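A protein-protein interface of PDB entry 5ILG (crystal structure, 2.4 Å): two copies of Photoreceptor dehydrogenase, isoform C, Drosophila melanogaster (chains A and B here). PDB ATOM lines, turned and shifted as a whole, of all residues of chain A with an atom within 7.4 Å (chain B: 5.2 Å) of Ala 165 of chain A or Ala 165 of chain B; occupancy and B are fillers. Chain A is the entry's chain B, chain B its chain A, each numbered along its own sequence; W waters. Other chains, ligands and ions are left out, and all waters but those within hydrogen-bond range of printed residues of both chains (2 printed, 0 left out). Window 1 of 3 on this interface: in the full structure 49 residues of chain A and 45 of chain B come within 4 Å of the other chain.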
ATOM      1  N   LEU A 117      -9.322  -6.203  -0.800  1.00  0.00           N
ATOM      2  CA  LEU A 117      -8.412  -5.270  -1.418  1.00  0.00           C
ATOM      3  C   LEU A 117      -8.638  -5.131  -2.928  1.00  0.00           C
ATOM      4  O   LEU A 117      -8.716  -4.020  -3.457  1.00  0.00           O
ATOM      5  CB  LEU A 117      -6.979  -5.656  -1.115  1.00  0.00           C
ATOM      6  CG  LEU A 117      -5.858  -4.723  -1.559  1.00  0.00           C
ATOM      7  CD1 LEU A 117      -6.170  -3.266  -1.280  1.00  0.00           C
ATOM      8  CD2 LEU A 117      -4.573  -5.132  -0.855  1.00  0.00           C
ATOM      9  N   SER A 146     -11.922   1.212   4.948  1.00  0.00           N
ATOM     10  CA  SER A 146     -10.827   0.565   5.665  1.00  0.00           C
ATOM     11  C   SER A 146     -11.301   0.189   7.071  1.00  0.00           C
ATOM     12  O   SER A 146     -12.471  -0.077   7.249  1.00  0.00           O
ATOM     13  CB  SER A 146      -9.564   1.445   5.673  1.00  0.00           C
ATOM     14  OG  SER A 146      -8.489   0.765   6.317  1.00  0.00           O
ATOM     15  N   SER A 147     -10.377   0.127   8.027  1.00  0.00           N
ATOM     16  CA  SER A 147     -10.679  -0.190   9.417  1.00  0.00           C
ATOM     17  C   SER A 147      -9.616   0.425  10.291  1.00  0.00           C
ATOM     18  O   SER A 147      -8.499   0.680   9.821  1.00  0.00           O
ATOM     19  CB  SER A 147     -10.663  -1.709   9.608  1.00  0.00           C
ATOM     20  OG  SER A 147     -10.717  -2.101  10.966  1.00  0.00           O
ATOM     21  N   VAL A 149      -7.977  -1.177  12.363  1.00  0.00           N
ATOM     22  CA  VAL A 149      -6.896  -2.189  12.368  1.00  0.00           C
ATOM     23  C   VAL A 149      -5.921  -2.070  11.198  1.00  0.00           C
ATOM     24  O   VAL A 149      -4.800  -2.568  11.267  1.00  0.00           O
ATOM     25  CB  VAL A 149      -7.419  -3.629  12.419  1.00  0.00           C
ATOM     26  CG1 VAL A 149      -8.481  -3.780  13.511  1.00  0.00           C
ATOM     27  CG2 VAL A 149      -7.958  -4.067  11.072  1.00  0.00           C
ATOM     28  N   GLY A 150      -6.376  -1.412  10.140  1.00  0.00           N
ATOM     29  CA  GLY A 150      -5.513  -0.961   9.040  1.00  0.00           C
ATOM     30  C   GLY A 150      -4.526   0.133   9.416  1.00  0.00           C
ATOM     31  O   GLY A 150      -3.446   0.259   8.833  1.00  0.00           O
ATOM     32  N   LEU A 151      -4.901   0.916  10.422  1.00  0.00           N
ATOM     33  CA  LEU A 151      -4.042   1.949  11.011  1.00  0.00           C
ATOM     34  C   LEU A 151      -3.126   1.368  12.088  1.00  0.00           C
ATOM     35  O   LEU A 151      -1.922   1.601  12.098  1.00  0.00           O
ATOM     36  CB  LEU A 151      -4.896   3.068  11.627  1.00  0.00           C
ATOM     37  CG  LEU A 151      -5.765   3.852  10.653  1.00  0.00           C
ATOM     38  CD1 LEU A 151      -6.792   4.676  11.414  1.00  0.00           C
ATOM     39  CD2 LEU A 151      -4.882   4.727   9.774  1.00  0.00           C
ATOM     40  N   PRO A 153      -2.327  -2.263  13.746  1.00  0.00           N
ATOM     41  CA  PRO A 153      -2.521  -3.691  13.603  1.00  0.00           C
ATOM     42  C   PRO A 153      -3.156  -4.346  14.831  1.00  0.00           C
ATOM     43  O   PRO A 153      -2.832  -4.010  15.958  1.00  0.00           O
ATOM     44  CB  PRO A 153      -1.097  -4.232  13.421  1.00  0.00           C
ATOM     45  CG  PRO A 153      -0.302  -3.067  12.976  1.00  0.00           C
ATOM     46  CD  PRO A 153      -0.904  -1.886  13.610  1.00  0.00           C
ATOM     47  N   VAL A 159      -4.373 -11.120   8.320  1.00  0.00           N
ATOM     48  CA  VAL A 159      -4.614 -11.085   6.844  1.00  0.00           C
ATOM     49  C   VAL A 159      -5.638 -10.010   6.478  1.00  0.00           C
ATOM     50  O   VAL A 159      -5.401  -9.164   5.628  1.00  0.00           O
ATOM     51  CB  VAL A 159      -5.018 -12.451   6.280  1.00  0.00           C
ATOM     52  CG1 VAL A 159      -5.259 -12.362   4.782  1.00  0.00           C
ATOM     53  CG2 VAL A 159      -3.924 -13.471   6.577  1.00  0.00           C
ATOM     54  N   TYR A 160      -6.773 -10.052   7.159  1.00  0.00           N
ATOM     55  CA  TYR A 160      -7.777  -8.970   7.118  1.00  0.00           C
ATOM     56  C   TYR A 160      -7.166  -7.586   7.282  1.00  0.00           C
ATOM     57  O   TYR A 160      -7.405  -6.691   6.486  1.00  0.00           O
ATOM     58  CB  TYR A 160      -8.828  -9.192   8.211  1.00  0.00           C
ATOM     59  CG  TYR A 160      -9.839  -8.098   8.344  1.00  0.00           C
ATOM     60  CD1 TYR A 160     -10.972  -8.066   7.540  1.00  0.00           C
ATOM     61  CD2 TYR A 160      -9.684  -7.097   9.286  1.00  0.00           C
ATOM     62  CE1 TYR A 160     -11.938  -7.043   7.671  1.00  0.00           C
ATOM     63  CE2 TYR A 160     -10.613  -6.055   9.412  1.00  0.00           C
ATOM     64  CZ  TYR A 160     -11.751  -6.036   8.621  1.00  0.00           C
ATOM     65  OH  TYR A 160     -12.681  -5.028   8.762  1.00  0.00           O
ATOM     66  N   GLY A 161      -6.330  -7.449   8.295  1.00  0.00           N
ATOM     67  CA  GLY A 161      -5.689  -6.185   8.619  1.00  0.00           C
ATOM     68  C   GLY A 161      -4.790  -5.665   7.529  1.00  0.00           C
ATOM     69  O   GLY A 161      -4.781  -4.450   7.188  1.00  0.00           O
ATOM     70  N   ALA A 162      -4.030  -6.581   6.969  1.00  0.00           N
ATOM     71  CA  ALA A 162      -3.189  -6.264   5.827  1.00  0.00           C
ATOM     72  C   ALA A 162      -4.008  -5.645   4.704  1.00  0.00           C
ATOM     73  O   ALA A 162      -3.591  -4.644   4.112  1.00  0.00           O
ATOM     74  CB  ALA A 162      -2.471  -7.515   5.337  1.00  0.00           C
ATOM     75  N   THR A 163      -5.169  -6.231   4.412  1.00  0.00           N
ATOM     76  CA  THR A 163      -6.015  -5.697   3.325  1.00  0.00           C
ATOM     77  C   THR A 163      -6.520  -4.322   3.704  1.00  0.00           C
ATOM     78  O   THR A 163      -6.712  -3.472   2.841  1.00  0.00           O
ATOM     79  CB  THR A 163      -7.215  -6.608   2.918  1.00  0.00           C
ATOM     80  OG1 THR A 163      -8.186  -6.704   3.982  1.00  0.00           O
ATOM     81  CG2 THR A 163      -6.728  -7.987   2.516  1.00  0.00           C
ATOM     82  N   LYS A 164      -6.765  -4.108   4.992  1.00  0.00           N
ATOM     83  CA  LYS A 164      -7.251  -2.802   5.451  1.00  0.00           C
ATOM     84  C   LYS A 164      -6.194  -1.737   5.357  1.00  0.00           C
ATOM     85  O   LYS A 164      -6.484  -0.608   5.037  1.00  0.00           O
ATOM     86  CB  LYS A 164      -7.841  -2.887   6.853  1.00  0.00           C
ATOM     87  CG  LYS A 164      -9.164  -3.660   6.898  1.00  0.00           C
ATOM     88  CD  LYS A 164     -10.285  -3.038   6.055  1.00  0.00           C
ATOM     89  CE  LYS A 164     -11.003  -4.064   5.205  1.00  0.00           C
ATOM     90  NZ  LYS A 164     -12.121  -3.481   4.362  1.00  0.00           N
ATOM     91  N   ALA A 165      -4.956  -2.106   5.650  1.00  0.00           N
ATOM     92  CA  ALA A 165      -3.829  -1.174   5.512  1.00  0.00           C
ATOM     93  C   ALA A 165      -3.606  -0.817   4.039  1.00  0.00           C
ATOM     94  O   ALA A 165      -3.345   0.328   3.699  1.00  0.00           O
ATOM     95  CB  ALA A 165      -2.569  -1.812   6.083  1.00  0.00           C
ATOM     96  N   GLY A 166      -3.743  -1.823   3.180  1.00  0.00           N
ATOM     97  CA  GLY A 166      -3.613  -1.599   1.757  1.00  0.00           C
ATOM     98  C   GLY A 166      -4.579  -0.589   1.204  1.00  0.00           C
ATOM     99  O   GLY A 166      -4.211   0.240   0.376  1.00  0.00           O
ATOM    100  N   ILE A 167      -5.829  -0.671   1.670  1.00  0.00           N
ATOM    101  CA  ILE A 167      -6.897   0.229   1.219  1.00  0.00           C
ATOM    102  C   ILE A 167      -6.550   1.674   1.499  1.00  0.00           C
ATOM    103  O   ILE A 167      -6.770   2.533   0.664  1.00  0.00           O
ATOM    104  CB  ILE A 167      -8.246  -0.137   1.853  1.00  0.00           C
ATOM    105  CG1 ILE A 167      -8.736  -1.492   1.317  1.00  0.00           C
ATOM    106  CG2 ILE A 167      -9.296   0.937   1.562  1.00  0.00           C
ATOM    107  CD1 ILE A 167      -9.790  -2.105   2.181  1.00  0.00           C
ATOM    108  N   ILE A 168      -6.002   1.924   2.681  1.00  0.00           N
ATOM    109  CA  ILE A 168      -5.585   3.262   3.076  1.00  0.00           C
ATOM    110  C   ILE A 168      -4.545   3.803   2.099  1.00  0.00           C
ATOM    111  O   ILE A 168      -4.705   4.861   1.506  1.00  0.00           O
ATOM    112  CB  ILE A 168      -4.993   3.285   4.502  1.00  0.00           C
ATOM    113  CG1 ILE A 168      -6.071   2.944   5.517  1.00  0.00           C
ATOM    114  CG2 ILE A 168      -4.412   4.657   4.831  1.00  0.00           C
ATOM    115  CD1 ILE A 168      -5.527   2.590   6.877  1.00  0.00           C
ATOM    116  N   ASN A 169      -3.467   3.042   1.932  1.00  0.00           N
ATOM    117  CA  ASN A 169      -2.365   3.418   1.032  1.00  0.00           C
ATOM    118  C   ASN A 169      -2.847   3.677  -0.389  1.00  0.00           C
ATOM    119  O   ASN A 169      -2.540   4.698  -0.982  1.00  0.00           O
ATOM    120  CB  ASN A 169      -1.298   2.338   1.041  1.00  0.00           C
ATOM    121  CG  ASN A 169      -0.015   2.790   0.403  1.00  0.00           C
ATOM    122  OD1 ASN A 169       0.065   2.894  -0.830  1.00  0.00           O
ATOM    123  ND2 ASN A 169       0.986   3.057   1.209  1.00  0.00           N
ATOM    124  N   PHE A 170      -3.641   2.760  -0.893  1.00  0.00           N
ATOM    125  CA  PHE A 170      -4.271   2.893  -2.216  1.00  0.00           C
ATOM    126  C   PHE A 170      -5.041   4.197  -2.347  1.00  0.00           C
ATOM    127  O   PHE A 170      -4.871   4.951  -3.297  1.00  0.00           O
ATOM    128  CB  PHE A 170      -5.207   1.706  -2.482  1.00  0.00           C
ATOM    129  CG  PHE A 170      -5.968   1.806  -3.770  1.00  0.00           C
ATOM    130  CD1 PHE A 170      -5.369   1.486  -4.988  1.00  0.00           C
ATOM    131  CD2 PHE A 170      -7.314   2.222  -3.777  1.00  0.00           C
ATOM    132  CE1 PHE A 170      -6.084   1.575  -6.195  1.00  0.00           C
ATOM    133  CE2 PHE A 170      -8.038   2.316  -4.980  1.00  0.00           C
ATOM    134  CZ  PHE A 170      -7.427   1.965  -6.192  1.00  0.00           C
ATOM    135  N   THR A 171      -5.907   4.436  -1.380  1.00  0.00           N
ATOM    136  CA  THR A 171      -6.829   5.562  -1.457  1.00  0.00           C
ATOM    137  C   THR A 171      -6.111   6.913  -1.295  1.00  0.00           C
ATOM    138  O   THR A 171      -6.372   7.864  -2.049  1.00  0.00           O
ATOM    139  CB  THR A 171      -7.957   5.390  -0.449  1.00  0.00           C
ATOM    140  OG1 THR A 171      -8.612   4.144  -0.715  1.00  0.00           O
ATOM    141  CG2 THR A 171      -8.970   6.528  -0.587  1.00  0.00           C
ATOM    142  N   SER B 146       8.956  -5.265   2.661  1.00  0.00           N
ATOM    143  CA  SER B 146       8.044  -4.174   2.329  1.00  0.00           C
ATOM    144  C   SER B 146       8.828  -3.142   1.524  1.00  0.00           C
ATOM    145  O   SER B 146       9.786  -3.474   0.860  1.00  0.00           O
ATOM    146  CB  SER B 146       7.397  -3.580   3.594  1.00  0.00           C
ATOM    147  OG  SER B 146       6.450  -2.569   3.236  1.00  0.00           O
ATOM    148  N   GLY B 150       5.253   1.749   1.232  1.00  0.00           N
ATOM    149  CA  GLY B 150       4.299   1.122   2.167  1.00  0.00           C
ATOM    150  C   GLY B 150       4.074   1.917   3.451  1.00  0.00           C
ATOM    151  O   GLY B 150       3.022   1.841   4.074  1.00  0.00           O
ATOM    152  N   GLY B 161       1.916  -0.210  -3.866  1.00  0.00           N
ATOM    153  CA  GLY B 161       2.061   0.408  -2.548  1.00  0.00           C
ATOM    154  C   GLY B 161       1.121  -0.175  -1.513  1.00  0.00           C
ATOM    155  O   GLY B 161       1.505  -0.438  -0.349  1.00  0.00           O
ATOM    156  N   ALA B 162      -0.108  -0.409  -1.946  1.00  0.00           N
ATOM    157  CA  ALA B 162      -1.107  -1.071  -1.108  1.00  0.00           C
ATOM    158  C   ALA B 162      -0.581  -2.402  -0.584  1.00  0.00           C
ATOM    159  O   ALA B 162      -0.721  -2.700   0.612  1.00  0.00           O
ATOM    160  CB  ALA B 162      -2.405  -1.290  -1.870  1.00  0.00           C
ATOM    161  N   THR B 163       0.019  -3.199  -1.472  1.00  0.00           N
ATOM    162  CA  THR B 163       0.557  -4.511  -1.062  1.00  0.00           C
ATOM    163  C   THR B 163       1.729  -4.325  -0.099  1.00  0.00           C
ATOM    164  O   THR B 163       1.905  -5.116   0.811  1.00  0.00           O
ATOM    165  CB  THR B 163       1.005  -5.432  -2.232  1.00  0.00           C
ATOM    166  OG1 THR B 163       2.170  -4.892  -2.908  1.00  0.00           O
ATOM    167  CG2 THR B 163      -0.142  -5.635  -3.222  1.00  0.00           C
ATOM    168  N   LYS B 164       2.514  -3.272  -0.302  1.00  0.00           N
ATOM    169  CA  LYS B 164       3.635  -2.983   0.606  1.00  0.00           C
ATOM    170  C   LYS B 164       3.179  -2.561   1.994  1.00  0.00           C
ATOM    171  O   LYS B 164       3.770  -2.929   2.995  1.00  0.00           O
ATOM    172  CB  LYS B 164       4.587  -1.947   0.003  1.00  0.00           C
ATOM    173  CG  LYS B 164       5.363  -2.502  -1.178  1.00  0.00           C
ATOM    174  CD  LYS B 164       6.222  -3.719  -0.831  1.00  0.00           C
ATOM    175  CE  LYS B 164       6.038  -4.842  -1.833  1.00  0.00           C
ATOM    176  NZ  LYS B 164       6.878  -6.041  -1.539  1.00  0.00           N
ATOM    177  N   ALA B 165       2.108  -1.797   2.042  1.00  0.00           N
ATOM    178  CA  ALA B 165       1.524  -1.395   3.328  1.00  0.00           C
ATOM    179  C   ALA B 165       0.960  -2.607   4.066  1.00  0.00           C
ATOM    180  O   ALA B 165       1.069  -2.748   5.271  1.00  0.00           O
ATOM    181  CB  ALA B 165       0.427  -0.357   3.081  1.00  0.00           C
ATOM    182  N   GLY B 166       0.314  -3.472   3.310  1.00  0.00           N
ATOM    183  CA  GLY B 166      -0.255  -4.684   3.867  1.00  0.00           C
ATOM    184  C   GLY B 166       0.754  -5.579   4.544  1.00  0.00           C
ATOM    185  O   GLY B 166       0.475  -6.147   5.608  1.00  0.00           O
ATOM    186  N   ILE B 167       1.915  -5.698   3.917  1.00  0.00           N
ATOM    187  CA  ILE B 167       2.986  -6.536   4.421  1.00  0.00           C
ATOM    188  C   ILE B 167       3.427  -6.075   5.819  1.00  0.00           C
ATOM    189  O   ILE B 167       3.682  -6.894   6.697  1.00  0.00           O
ATOM    190  CB  ILE B 167       4.200  -6.543   3.462  1.00  0.00           C
ATOM    191  CG1 ILE B 167       3.834  -7.256   2.176  1.00  0.00           C
ATOM    192  CG2 ILE B 167       5.431  -7.220   4.112  1.00  0.00           C
ATOM    193  CD1 ILE B 167       4.790  -6.949   1.059  1.00  0.00           C
ATOM    194  N   ILE B 168       3.514  -4.770   6.004  1.00  0.00           N
ATOM    195  CA  ILE B 168       3.881  -4.190   7.285  1.00  0.00           C
ATOM    196  C   ILE B 168       2.865  -4.600   8.381  1.00  0.00           C
ATOM    197  O   ILE B 168       3.208  -5.159   9.415  1.00  0.00           O
ATOM    198  CB  ILE B 168       3.954  -2.653   7.208  1.00  0.00           C
ATOM    199  CG1 ILE B 168       5.083  -2.212   6.296  1.00  0.00           C
ATOM    200  CG2 ILE B 168       4.180  -2.055   8.594  1.00  0.00           C
ATOM    201  CD1 ILE B 168       4.969  -0.766   5.877  1.00  0.00           C
ATOM    202  N   ASN B 169       1.609  -4.317   8.112  1.00  0.00           N
ATOM    203  CA  ASN B 169       0.533  -4.635   9.058  1.00  0.00           C
ATOM    204  C   ASN B 169       0.516  -6.119   9.435  1.00  0.00           C
ATOM    205  O   ASN B 169       0.474  -6.487  10.608  1.00  0.00           O
ATOM    206  CB  ASN B 169      -0.796  -4.199   8.472  1.00  0.00           C
ATOM    207  CG  ASN B 169      -1.905  -4.298   9.461  1.00  0.00           C
ATOM    208  OD1 ASN B 169      -2.338  -5.402   9.819  1.00  0.00           O
ATOM    209  ND2 ASN B 169      -2.364  -3.156   9.945  1.00  0.00           N
HETATM  210  O   HOH W   1       0.463   3.198   4.236  1.00  0.00           O
HETATM  211  O   HOH W   2      -0.445  -0.938   9.388  1.00  0.00           O
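Leu 117 of chain A touches none of the printed residues of chain B. Of the printed residues of chain B, Val 149 of chain A touches Asn 169 (2.8 Å). Ala 165 of chain A touches two residues of chain B. Of the printed residues of chain B, Asn 169 of chain A touches Gly 150, Gly 161, Ala 162 and Ala 165. Lys 164 of chain B touches none of the printed residues of chain A. Of chain A, only Ala 165 and Asn 169 come within 4 Å of Ala 165 of chain B. The nearest residue of chain B that does not touch Ala 165 of chain A is Gly 166 of chain B (4.3 Å). The nearest residue of chain A that does not touch Ala 165 of chain B is Gly 166 of chain A (4.4 Å). The nearest printed residue of chain A that does not touch Gly 150 of chain B is Ala 165 of chain A (6.6 Å).
The side-chain amide oxygen of Asn 169 of chain A is in hydrogen-bond range of the backbone NH of Ala 162 of chain B (3.5 Å). ND2 of Asn 169 of chain B sits at hydrogen-bond distance from O of Val 149 of chain A.
Water W1 bridges the backbone carbonyl oxygen of Gly 150 of chain B (2.9 Å) and the side-chain amide nitrogen of Asn 169 of chain A (3.1 Å). Water W2 lies within hydrogen-bond range of ND2 of Asn 169 of chain B (3.0 Å) and O of Gly 150 of chain A (3.3 Å).
Hydrophobic or aromatic side chains of chain A that line the printed part of chain B: Pro 153, Ala 162 and Ala 165. Of the 11 printed residues of chain B, 6 touch a printed residue of chain A. Hydrophobic or aromatic side chains of chain B that line the printed part of chain A: Ala 162 and Ala 165. Among the printed residues, 13 pairs touch across the chains. Among the printed residues, no Asp or Glu carboxylate lies within 4 Å of a Lys or Arg side-chain nitrogen of the other chain.
Gly 150 of chain A touches Asn 169 of chain B, and with the chains exchanged Asn 169 of chain A touches Gly 150 of chain B. Ala 162 of chain A touches Gly 166 of chain B, and with the chains exchanged Gly 166 of chain A touches Ala 162 of chain B. Ala 165 of chain B touches its own counterpart, Ala 165 of chain A. Ala 165 of chain A touches Asn 169 of chain B, and with the chains exchanged Asn 169 of chain A touches Ala 165 of chain B. 11 positions are printed for both chains. Of the 13 pairs that touch across the chains among the printed residues, 11 have their exchanged pair printed and touching as well.
Among the printed residues, pairs that only touch across the chains: Ala 162 of chain A with Gly 166 of chain B (3.3 Å), Gly 166 of chain A with Ala 162 of chain B (3.3 Å), Asn 169 of chain A with Gly 161 of chain B (3.3 Å), Gly 161 of chain A with Asn 169 of chain B (3.4 Å), Ala 162 of chain A with Asn 169 of chain B (3.5 Å), Pro 153 of chain A with Asn 169 of chain B (3.7 Å), Asn 169 of chain A with Gly 150 of chain B (3.7 Å), Gly 150 of chain A with Asn 169 of chain B (3.8 Å), Asn 169 of chain A with Ala 165 of chain B (3.8 Å), Ala 165 of chain A with Asn 169 of chain B (3.8 Å) and Ala 165 of chain A with Ala 165 of chain B (3.8 Å).
The backbone NH of Val 149 of chain A lies close to the side-chain hydroxyl of Ser 147 of chain A (3.2 Å).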
